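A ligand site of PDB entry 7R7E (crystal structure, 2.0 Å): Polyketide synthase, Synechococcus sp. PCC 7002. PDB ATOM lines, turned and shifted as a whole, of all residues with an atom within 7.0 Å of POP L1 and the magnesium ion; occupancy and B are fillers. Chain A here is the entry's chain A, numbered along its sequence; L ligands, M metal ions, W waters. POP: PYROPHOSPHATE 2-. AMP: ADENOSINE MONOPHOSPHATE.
NZ of Lys 550 is in salt-bridge range of O6 of POP L1.
The backbone NH (N) of Ser 174 lies within hydrogen-bond range of an oxygen (O) of POP L1 (3.2 Å).
NH2 of Arg 451 is in salt-bridge range of O6 of POP L1 (3.0 Å).
The backbone NH (N) of Thr 175 sits at hydrogen-bond distance from an oxygen (O3) of POP L1 (2.8 Å).
An oxygen (O3) of POP L1 is in hydrogen-bond range of the side-chain hydroxyl (OG1) of Thr 175, 2.7 Å away.
The side-chain amino group of Lys 550 lies within salt-bridge range of an oxygen (O1P) of AMP L2 (2.9 Å).
The side-chain carboxylate of Asp 437 lies within hydrogen-bond range of an oxygen (O3') of AMP L2 (2.6 Å).
The side-chain carboxylate (OD2) of Asp 216 lies close to an oxygen (O2P) of AMP L2 (2.9 Å).
The backbone NH (N) of Gly 173 lies within hydrogen-bond range of an oxygen (O1) of POP L1, 2.8 Å away.
NE of Arg 451 sits close to O2' of AMP L2 (3.4 Å).
The backbone NH of Ala 326 is in hydrogen-bond range of an oxygen (O3P) of AMP L2 (3.0 Å).
The side-chain hydroxyl of Thr 171 sits at hydrogen-bond distance from an oxygen (O1) of POP L1 (2.7 Å).
The side-chain hydroxyl (OG) of Ser 174 is in hydrogen-bond range of an oxygen (O6) of POP L1 (2.9 Å).
A nitrogen (N7) of AMP L2 is in hydrogen-bond range of the backbone NH (N) of Ala 294, at 3.2 Å.
The side-chain amino group (NZ) of Lys 179 lies within salt-bridge range of an oxygen (O1) of POP L1.
N of Ser 172 is in hydrogen-bond range of O4 of POP L1, 2.9 Å away.
O4 of POP L1 sits close to O1P of AMP L2 (2.9 Å).
The backbone carbonyl oxygen of Ser 174 lies within hydrogen-bond range of a ring nitrogen (ND1) of His 554, 3.2 Å away.
O of Lys 179 lies within hydrogen-bond range of N of Thr 171.
N of Lys 550 is in hydrogen-bond range of OG1 of Thr 546, at 3.1 Å.
The side-chain amino group (NZ) of Lys 550 is in hydrogen-bond range of the side-chain hydroxyl (OG) of Ser 172, 2.8 Å away.
Within 4 Å of POP L1: Thr 171, Ser 172, Gly 173, Ser 174, Thr 175, Lys 179, Arg 451 and Lys 550.
Arg 451 touches the magnesium ion.
The nearest printed residue that does not touch the magnesium ion is Glu 327 (4.2 Å).
O2 of POP L1 is bound to the magnesium ion (2.1 Å).
O5 of POP L1 is bound to the magnesium ion (2.1 Å).
Water W3 binds the magnesium ion, 2.2 Å away.
Water W2 binds the magnesium ion (2.2 Å).
Water W1 binds the magnesium ion (2.3 Å).
The magnesium ion is bound by water W4 (2.4 Å).
Water W1 lies within hydrogen-bond range of an oxygen (O3P) of AMP L2, the side-chain carboxylate (OE1) of Glu 327 and an oxygen (O4) of POP L1.
Water W4 lies within hydrogen-bond range of O3 of POP L1, OG1 of Thr 175 and NH1 of Arg 451.
Water W5 lies within hydrogen-bond range of O of Asp 177 (2.5 Å), NZ of Lys 179 (2.6 Å), O1 of POP L1 (2.7 Å) and O of Gly 176 (3.3 Å).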
ATOM      1  N   TYR A 170     -25.966 -19.432  33.401  1.00  0.00           N
ATOM      2  CA  TYR A 170     -25.395 -19.941  32.135  1.00  0.00           C
ATOM      3  C   TYR A 170     -25.489 -21.466  32.096  1.00  0.00           C
ATOM      4  O   TYR A 170     -25.167 -22.101  33.103  1.00  0.00           O
ATOM      5  CB  TYR A 170     -24.002 -19.385  31.872  1.00  0.00           C
ATOM      6  CG  TYR A 170     -24.009 -18.045  31.186  1.00  0.00           C
ATOM      7  CD1 TYR A 170     -24.233 -16.886  31.907  1.00  0.00           C
ATOM      8  CD2 TYR A 170     -23.811 -17.925  29.823  1.00  0.00           C
ATOM      9  CE1 TYR A 170     -24.263 -15.648  31.295  1.00  0.00           C
ATOM     10  CE2 TYR A 170     -23.832 -16.695  29.190  1.00  0.00           C
ATOM     11  CZ  TYR A 170     -24.060 -15.551  29.930  1.00  0.00           C
ATOM     12  OH  TYR A 170     -24.082 -14.331  29.347  1.00  0.00           O
ATOM     13  N   THR A 171     -25.937 -21.994  30.964  1.00  0.00           N
ATOM     14  CA  THR A 171     -26.004 -23.429  30.753  1.00  0.00           C
ATOM     15  C   THR A 171     -24.589 -23.976  30.682  1.00  0.00           C
ATOM     16  O   THR A 171     -23.617 -23.210  30.589  1.00  0.00           O
ATOM     17  CB  THR A 171     -26.739 -23.775  29.440  1.00  0.00           C
ATOM     18  OG1 THR A 171     -25.955 -23.350  28.309  1.00  0.00           O
ATOM     19  CG2 THR A 171     -28.097 -23.087  29.365  1.00  0.00           C
ATOM     20  N   SER A 172     -24.471 -25.306  30.745  1.00  0.00           N
ATOM     21  CA  SER A 172     -23.161 -25.909  30.953  1.00  0.00           C
ATOM     22  C   SER A 172     -22.280 -25.806  29.724  1.00  0.00           C
ATOM     23  O   SER A 172     -21.053 -25.808  29.835  1.00  0.00           O
ATOM     24  CB  SER A 172     -23.294 -27.391  31.380  1.00  0.00           C
ATOM     25  OG  SER A 172     -23.865 -27.491  32.680  1.00  0.00           O
ATOM     26  N   GLY A 173     -22.886 -25.747  28.545  1.00  0.00           N
ATOM     27  CA  GLY A 173     -22.135 -25.865  27.337  1.00  0.00           C
ATOM     28  C   GLY A 173     -22.081 -27.266  26.795  1.00  0.00           C
ATOM     29  O   GLY A 173     -21.197 -27.567  25.970  1.00  0.00           O
ATOM     30  N   SER A 174     -22.987 -28.146  27.224  1.00  0.00           N
ATOM     31  CA  SER A 174     -22.922 -29.549  26.782  1.00  0.00           C
ATOM     32  C   SER A 174     -23.106 -29.680  25.264  1.00  0.00           C
ATOM     33  O   SER A 174     -22.420 -30.486  24.619  1.00  0.00           O
ATOM     34  CB  SER A 174     -23.982 -30.390  27.486  1.00  0.00           C
ATOM     35  OG  SER A 174     -23.776 -30.399  28.890  1.00  0.00           O
ATOM     36  N   THR A 175     -24.069 -28.954  24.701  1.00  0.00           N
ATOM     37  CA  THR A 175     -24.439 -29.092  23.283  1.00  0.00           C
ATOM     38  C   THR A 175     -24.023 -27.884  22.448  1.00  0.00           C
ATOM     39  O   THR A 175     -24.305 -27.849  21.257  1.00  0.00           O
ATOM     40  CB  THR A 175     -25.949 -29.321  23.140  1.00  0.00           C
ATOM     41  OG1 THR A 175     -26.644 -28.147  23.567  1.00  0.00           O
ATOM     42  CG2 THR A 175     -26.429 -30.517  24.010  1.00  0.00           C
ATOM     43  N   GLY A 176     -23.417 -26.860  23.043  1.00  0.00           N
ATOM     44  CA  GLY A 176     -23.019 -25.689  22.286  1.00  0.00           C
ATOM     45  C   GLY A 176     -22.497 -24.667  23.266  1.00  0.00           C
ATOM     46  O   GLY A 176     -22.246 -24.988  24.424  1.00  0.00           O
ATOM     47  N   ASP A 177     -22.351 -23.426  22.797  1.00  0.00           N
ATOM     48  CA  ASP A 177     -21.873 -22.376  23.687  1.00  0.00           C
ATOM     49  C   ASP A 177     -22.825 -22.210  24.872  1.00  0.00           C
ATOM     50  O   ASP A 177     -24.049 -22.316  24.707  1.00  0.00           O
ATOM     51  CB  ASP A 177     -21.736 -21.057  22.936  1.00  0.00           C
ATOM     52  CG  ASP A 177     -20.342 -20.869  22.351  1.00  0.00           C
ATOM     53  OD1 ASP A 177     -19.780 -21.871  21.861  1.00  0.00           O
ATOM     54  OD2 ASP A 177     -19.808 -19.724  22.414  1.00  0.00           O
ATOM     55  N   PRO A 178     -22.297 -21.966  26.085  1.00  0.00           N
ATOM     56  CA  PRO A 178     -23.191 -21.616  27.206  1.00  0.00           C
ATOM     57  C   PRO A 178     -24.074 -20.421  26.863  1.00  0.00           C
ATOM     58  O   PRO A 178     -23.597 -19.388  26.383  1.00  0.00           O
ATOM     59  CB  PRO A 178     -22.215 -21.316  28.360  1.00  0.00           C
ATOM     60  CG  PRO A 178     -21.009 -22.223  28.054  1.00  0.00           C
ATOM     61  CD  PRO A 178     -20.892 -22.126  26.522  1.00  0.00           C
ATOM     62  N   LYS A 179     -25.366 -20.568  27.096  1.00  0.00           N
ATOM     63  CA  LYS A 179     -26.356 -19.511  26.878  1.00  0.00           C
ATOM     64  C   LYS A 179     -26.834 -18.966  28.215  1.00  0.00           C
ATOM     65  O   LYS A 179     -26.947 -19.713  29.201  1.00  0.00           O
ATOM     66  CB  LYS A 179     -27.549 -20.043  26.092  1.00  0.00           C
ATOM     67  CG  LYS A 179     -27.219 -21.077  25.072  1.00  0.00           C
ATOM     68  CD  LYS A 179     -28.499 -21.762  24.661  1.00  0.00           C
ATOM     69  CE  LYS A 179     -28.821 -22.978  25.553  1.00  0.00           C
ATOM     70  NZ  LYS A 179     -28.050 -24.243  25.156  1.00  0.00           N
ATOM     71  N   ASP A 216     -27.535 -24.315  38.726  1.00  0.00           N
ATOM     72  CA  ASP A 216     -28.873 -24.574  39.316  1.00  0.00           C
ATOM     73  C   ASP A 216     -28.932 -25.542  40.499  1.00  0.00           C
ATOM     74  O   ASP A 216     -29.439 -25.115  41.546  1.00  0.00           O
ATOM     75  CB  ASP A 216     -29.893 -24.953  38.233  1.00  0.00           C
ATOM     76  CG  ASP A 216     -29.338 -25.875  37.156  1.00  0.00           C
ATOM     77  OD1 ASP A 216     -28.506 -26.744  37.493  1.00  0.00           O
ATOM     78  OD2 ASP A 216     -29.746 -25.721  35.992  1.00  0.00           O
ATOM     79  N   ALA A 294     -30.102 -34.220  36.977  1.00  0.00           N
ATOM     80  CA  ALA A 294     -29.020 -33.574  36.195  1.00  0.00           C
ATOM     81  C   ALA A 294     -28.421 -34.555  35.189  1.00  0.00           C
ATOM     82  O   ALA A 294     -27.619 -34.125  34.356  1.00  0.00           O
ATOM     83  CB  ALA A 294     -27.979 -32.928  37.052  1.00  0.00           C
ATOM     84  N   MET A 325     -34.058 -28.168  34.501  1.00  0.00           N
ATOM     85  CA  MET A 325     -33.006 -27.537  33.723  1.00  0.00           C
ATOM     86  C   MET A 325     -32.917 -26.046  34.061  1.00  0.00           C
ATOM     87  O   MET A 325     -33.835 -25.465  34.645  1.00  0.00           O
ATOM     88  CB  MET A 325     -33.284 -27.818  32.264  1.00  0.00           C
ATOM     89  CG  MET A 325     -34.438 -27.034  31.773  1.00  0.00           C
ATOM     90  SD  MET A 325     -35.072 -27.627  30.158  1.00  0.00           S
ATOM     91  CE  MET A 325     -33.580 -27.692  29.060  1.00  0.00           C
ATOM     92  N   ALA A 326     -31.847 -25.410  33.581  1.00  0.00           N
ATOM     93  CA  ALA A 326     -31.652 -24.000  33.893  1.00  0.00           C
ATOM     94  C   ALA A 326     -32.796 -23.171  33.345  1.00  0.00           C
ATOM     95  O   ALA A 326     -33.299 -22.267  34.031  1.00  0.00           O
ATOM     96  CB  ALA A 326     -30.308 -23.506  33.366  1.00  0.00           C
ATOM     97  N   GLU A 327     -33.272 -23.508  32.125  1.00  0.00           N
ATOM     98  CA  GLU A 327     -34.377 -22.785  31.466  1.00  0.00           C
ATOM     99  C   GLU A 327     -35.696 -22.893  32.244  1.00  0.00           C
ATOM    100  O   GLU A 327     -36.614 -22.081  32.036  1.00  0.00           O
ATOM    101  CB  GLU A 327     -34.615 -23.300  30.011  1.00  0.00           C
ATOM    102  CG  GLU A 327     -33.539 -22.886  28.996  1.00  0.00           C
ATOM    103  CD  GLU A 327     -32.385 -23.899  28.934  1.00  0.00           C
ATOM    104  OE1 GLU A 327     -32.277 -24.739  29.888  1.00  0.00           O
ATOM    105  OE2 GLU A 327     -31.642 -23.884  27.895  1.00  0.00           O
ATOM    106  N   TYR A 411     -33.339 -16.320  26.668  1.00  0.00           N
ATOM    107  CA  TYR A 411     -31.877 -16.313  26.642  1.00  0.00           C
ATOM    108  C   TYR A 411     -31.405 -14.890  26.463  1.00  0.00           C
ATOM    109  O   TYR A 411     -31.832 -14.210  25.522  1.00  0.00           O
ATOM    110  CB  TYR A 411     -31.352 -17.147  25.488  1.00  0.00           C
ATOM    111  CG  TYR A 411     -31.645 -18.598  25.596  1.00  0.00           C
ATOM    112  CD1 TYR A 411     -31.424 -19.314  26.769  1.00  0.00           C
ATOM    113  CD2 TYR A 411     -32.173 -19.265  24.493  1.00  0.00           C
ATOM    114  CE1 TYR A 411     -31.708 -20.701  26.845  1.00  0.00           C
ATOM    115  CE2 TYR A 411     -32.458 -20.596  24.555  1.00  0.00           C
ATOM    116  CZ  TYR A 411     -32.211 -21.319  25.690  1.00  0.00           C
ATOM    117  OH  TYR A 411     -32.545 -22.660  25.647  1.00  0.00           O
ATOM    118  N   THR A 435     -37.665 -27.907  25.628  1.00  0.00           N
ATOM    119  CA  THR A 435     -36.523 -28.268  26.476  1.00  0.00           C
ATOM    120  C   THR A 435     -35.349 -28.800  25.685  1.00  0.00           C
ATOM    121  O   THR A 435     -34.211 -28.749  26.182  1.00  0.00           O
ATOM    122  CB  THR A 435     -36.908 -29.324  27.518  1.00  0.00           C
ATOM    123  OG1 THR A 435     -37.312 -30.552  26.867  1.00  0.00           O
ATOM    124  CG2 THR A 435     -37.993 -28.795  28.454  1.00  0.00           C
ATOM    125  N   ASP A 437     -35.167 -31.958  25.303  1.00  0.00           N
ATOM    126  CA  ASP A 437     -35.066 -33.315  25.790  1.00  0.00           C
ATOM    127  C   ASP A 437     -36.160 -34.173  25.166  1.00  0.00           C
ATOM    128  O   ASP A 437     -37.283 -33.710  24.945  1.00  0.00           O
ATOM    129  CB  ASP A 437     -35.142 -33.370  27.326  1.00  0.00           C
ATOM    130  CG  ASP A 437     -33.984 -32.628  27.995  1.00  0.00           C
ATOM    131  OD1 ASP A 437     -32.813 -32.947  27.663  1.00  0.00           O
ATOM    132  OD2 ASP A 437     -34.230 -31.797  28.924  1.00  0.00           O
ATOM    133  N   ARG A 451     -31.157 -36.276  25.025  1.00  0.00           N
ATOM    134  CA  ARG A 451     -31.098 -34.961  24.400  1.00  0.00           C
ATOM    135  C   ARG A 451     -31.333 -35.097  22.911  1.00  0.00           C
ATOM    136  O   ARG A 451     -30.750 -35.966  22.277  1.00  0.00           O
ATOM    137  CB  ARG A 451     -29.759 -34.254  24.638  1.00  0.00           C
ATOM    138  CG  ARG A 451     -29.233 -34.419  26.068  1.00  0.00           C
ATOM    139  CD  ARG A 451     -28.047 -33.481  26.291  1.00  0.00           C
ATOM    140  NE  ARG A 451     -27.725 -33.322  27.712  1.00  0.00           N
ATOM    141  CZ  ARG A 451     -27.596 -32.155  28.331  1.00  0.00           C
ATOM    142  NH1 ARG A 451     -27.824 -31.012  27.704  1.00  0.00           N
ATOM    143  NH2 ARG A 451     -27.216 -32.146  29.610  1.00  0.00           N
ATOM    144  N   THR A 546     -17.396 -29.926  30.053  1.00  0.00           N
ATOM    145  CA  THR A 546     -17.761 -28.679  30.694  1.00  0.00           C
ATOM    146  C   THR A 546     -17.010 -28.546  32.030  1.00  0.00           C
ATOM    147  O   THR A 546     -16.319 -29.459  32.481  1.00  0.00           O
ATOM    148  CB  THR A 546     -19.267 -28.598  30.931  1.00  0.00           C
ATOM    149  OG1 THR A 546     -19.668 -29.528  31.943  1.00  0.00           O
ATOM    150  CG2 THR A 546     -20.058 -28.915  29.621  1.00  0.00           C
ATOM    151  N   SER A 548     -18.346 -28.479  34.959  1.00  0.00           N
ATOM    152  CA  SER A 548     -18.934 -29.498  35.827  1.00  0.00           C
ATOM    153  C   SER A 548     -18.520 -30.918  35.440  1.00  0.00           C
ATOM    154  O   SER A 548     -18.893 -31.867  36.137  1.00  0.00           O
ATOM    155  CB  SER A 548     -20.454 -29.372  35.776  1.00  0.00           C
ATOM    156  OG  SER A 548     -20.882 -29.225  34.418  1.00  0.00           O
ATOM    157  N   LYS A 550     -19.360 -32.547  32.480  1.00  0.00           N
ATOM    158  CA  LYS A 550     -20.169 -33.193  31.446  1.00  0.00           C
ATOM    159  C   LYS A 550     -19.430 -33.240  30.120  1.00  0.00           C
ATOM    160  O   LYS A 550     -18.839 -32.254  29.696  1.00  0.00           O
ATOM    161  CB  LYS A 550     -21.496 -32.464  31.231  1.00  0.00           C
ATOM    162  CG  LYS A 550     -22.336 -32.243  32.474  1.00  0.00           C
ATOM    163  CD  LYS A 550     -23.526 -31.361  32.107  1.00  0.00           C
ATOM    164  CE  LYS A 550     -24.316 -30.929  33.332  1.00  0.00           C
ATOM    165  NZ  LYS A 550     -25.335 -29.869  33.054  1.00  0.00           N
ATOM    166  N   HIS A 554     -20.469 -32.711  20.921  1.00  0.00           N
ATOM    167  CA  HIS A 554     -20.209 -31.914  19.725  1.00  0.00           C
ATOM    168  C   HIS A 554     -18.733 -31.496  19.613  1.00  0.00           C
ATOM    169  O   HIS A 554     -18.198 -31.477  18.506  1.00  0.00           O
ATOM    170  CB  HIS A 554     -21.143 -30.679  19.717  1.00  0.00           C
ATOM    171  CG  HIS A 554     -20.761 -29.611  20.716  1.00  0.00           C
ATOM    172  ND1 HIS A 554     -20.657 -29.838  22.076  1.00  0.00           N
ATOM    173  CD2 HIS A 554     -20.457 -28.293  20.529  1.00  0.00           C
ATOM    174  CE1 HIS A 554     -20.298 -28.722  22.687  1.00  0.00           C
ATOM    175  NE2 HIS A 554     -20.170 -27.772  21.776  1.00  0.00           N
HETATM  176  P1  POP L   1     -26.226 -26.807  27.384  1.00  0.00           P
HETATM  177  O1  POP L   1     -25.290 -25.683  27.198  1.00  0.00           O
HETATM  178  O2  POP L   1     -27.627 -26.304  27.550  1.00  0.00           O
HETATM  179  O3  POP L   1     -26.094 -27.615  26.148  1.00  0.00           O
HETATM  180  O   POP L   1     -25.805 -27.775  28.590  1.00  0.00           O
HETATM  181  P2  POP L   1     -26.743 -28.237  29.781  1.00  0.00           P
HETATM  182  O4  POP L   1     -26.787 -27.098  30.754  1.00  0.00           O
HETATM  183  O5  POP L   1     -28.124 -28.580  29.336  1.00  0.00           O
HETATM  184  O6  POP L   1     -26.125 -29.455  30.377  1.00  0.00           O
HETATM  185  P   AMP L   2     -28.839 -27.970  33.353  1.00  0.00           P
HETATM  186  O1P AMP L   2     -27.357 -27.863  33.468  1.00  0.00           O
HETATM  187  O2P AMP L   2     -29.533 -28.262  34.637  1.00  0.00           O
HETATM  188  O3P AMP L   2     -29.491 -26.909  32.542  1.00  0.00           O
HETATM  189  O5' AMP L   2     -29.010 -29.305  32.493  1.00  0.00           O
HETATM  190  C5' AMP L   2     -30.302 -29.751  32.103  1.00  0.00           C
HETATM  191  C4' AMP L   2     -30.203 -31.073  31.377  1.00  0.00           C
HETATM  192  O4' AMP L   2     -29.719 -32.136  32.190  1.00  0.00           O
HETATM  193  C3' AMP L   2     -31.568 -31.542  30.961  1.00  0.00           C
HETATM  194  O3' AMP L   2     -31.989 -30.857  29.813  1.00  0.00           O
HETATM  195  C2' AMP L   2     -31.303 -32.986  30.683  1.00  0.00           C
HETATM  196  O2' AMP L   2     -30.662 -33.142  29.422  1.00  0.00           O
HETATM  197  C1' AMP L   2     -30.332 -33.360  31.777  1.00  0.00           C
HETATM  198  N9  AMP L   2     -31.162 -33.932  32.840  1.00  0.00           N
HETATM  199  C8  AMP L   2     -31.599 -33.319  33.953  1.00  0.00           C
HETATM  200  N7  AMP L   2     -32.353 -34.134  34.708  1.00  0.00           N
HETATM  201  C5  AMP L   2     -32.417 -35.296  34.057  1.00  0.00           C
HETATM  202  C6  AMP L   2     -33.069 -36.579  34.302  1.00  0.00           C
HETATM  203  N6  AMP L   2     -33.794 -36.769  35.414  1.00  0.00           N
HETATM  204  N1  AMP L   2     -32.908 -37.544  33.378  1.00  0.00           N
HETATM  205  C2  AMP L   2     -32.187 -37.342  32.273  1.00  0.00           C
HETATM  206  N3  AMP L   2     -31.561 -36.196  31.983  1.00  0.00           N
HETATM  207  C4  AMP L   2     -31.643 -35.159  32.832  1.00  0.00           C
HETATM  208 MG    MG M   1     -29.302 -27.378  28.100  1.00  0.00          MG
HETATM  209  O   HOH W   1     -30.010 -26.336  29.980  1.00  0.00           O
HETATM  210  O   HOH W   2     -30.756 -28.994  28.559  1.00  0.00           O
HETATM  211  O   HOH W   3     -30.566 -25.969  26.999  1.00  0.00           O
HETATM  212  O   HOH W   4     -28.601 -28.390  25.984  1.00  0.00           O
HETATM  213  O   HOH W   5     -25.449 -24.363  24.835  1.00  0.00           O
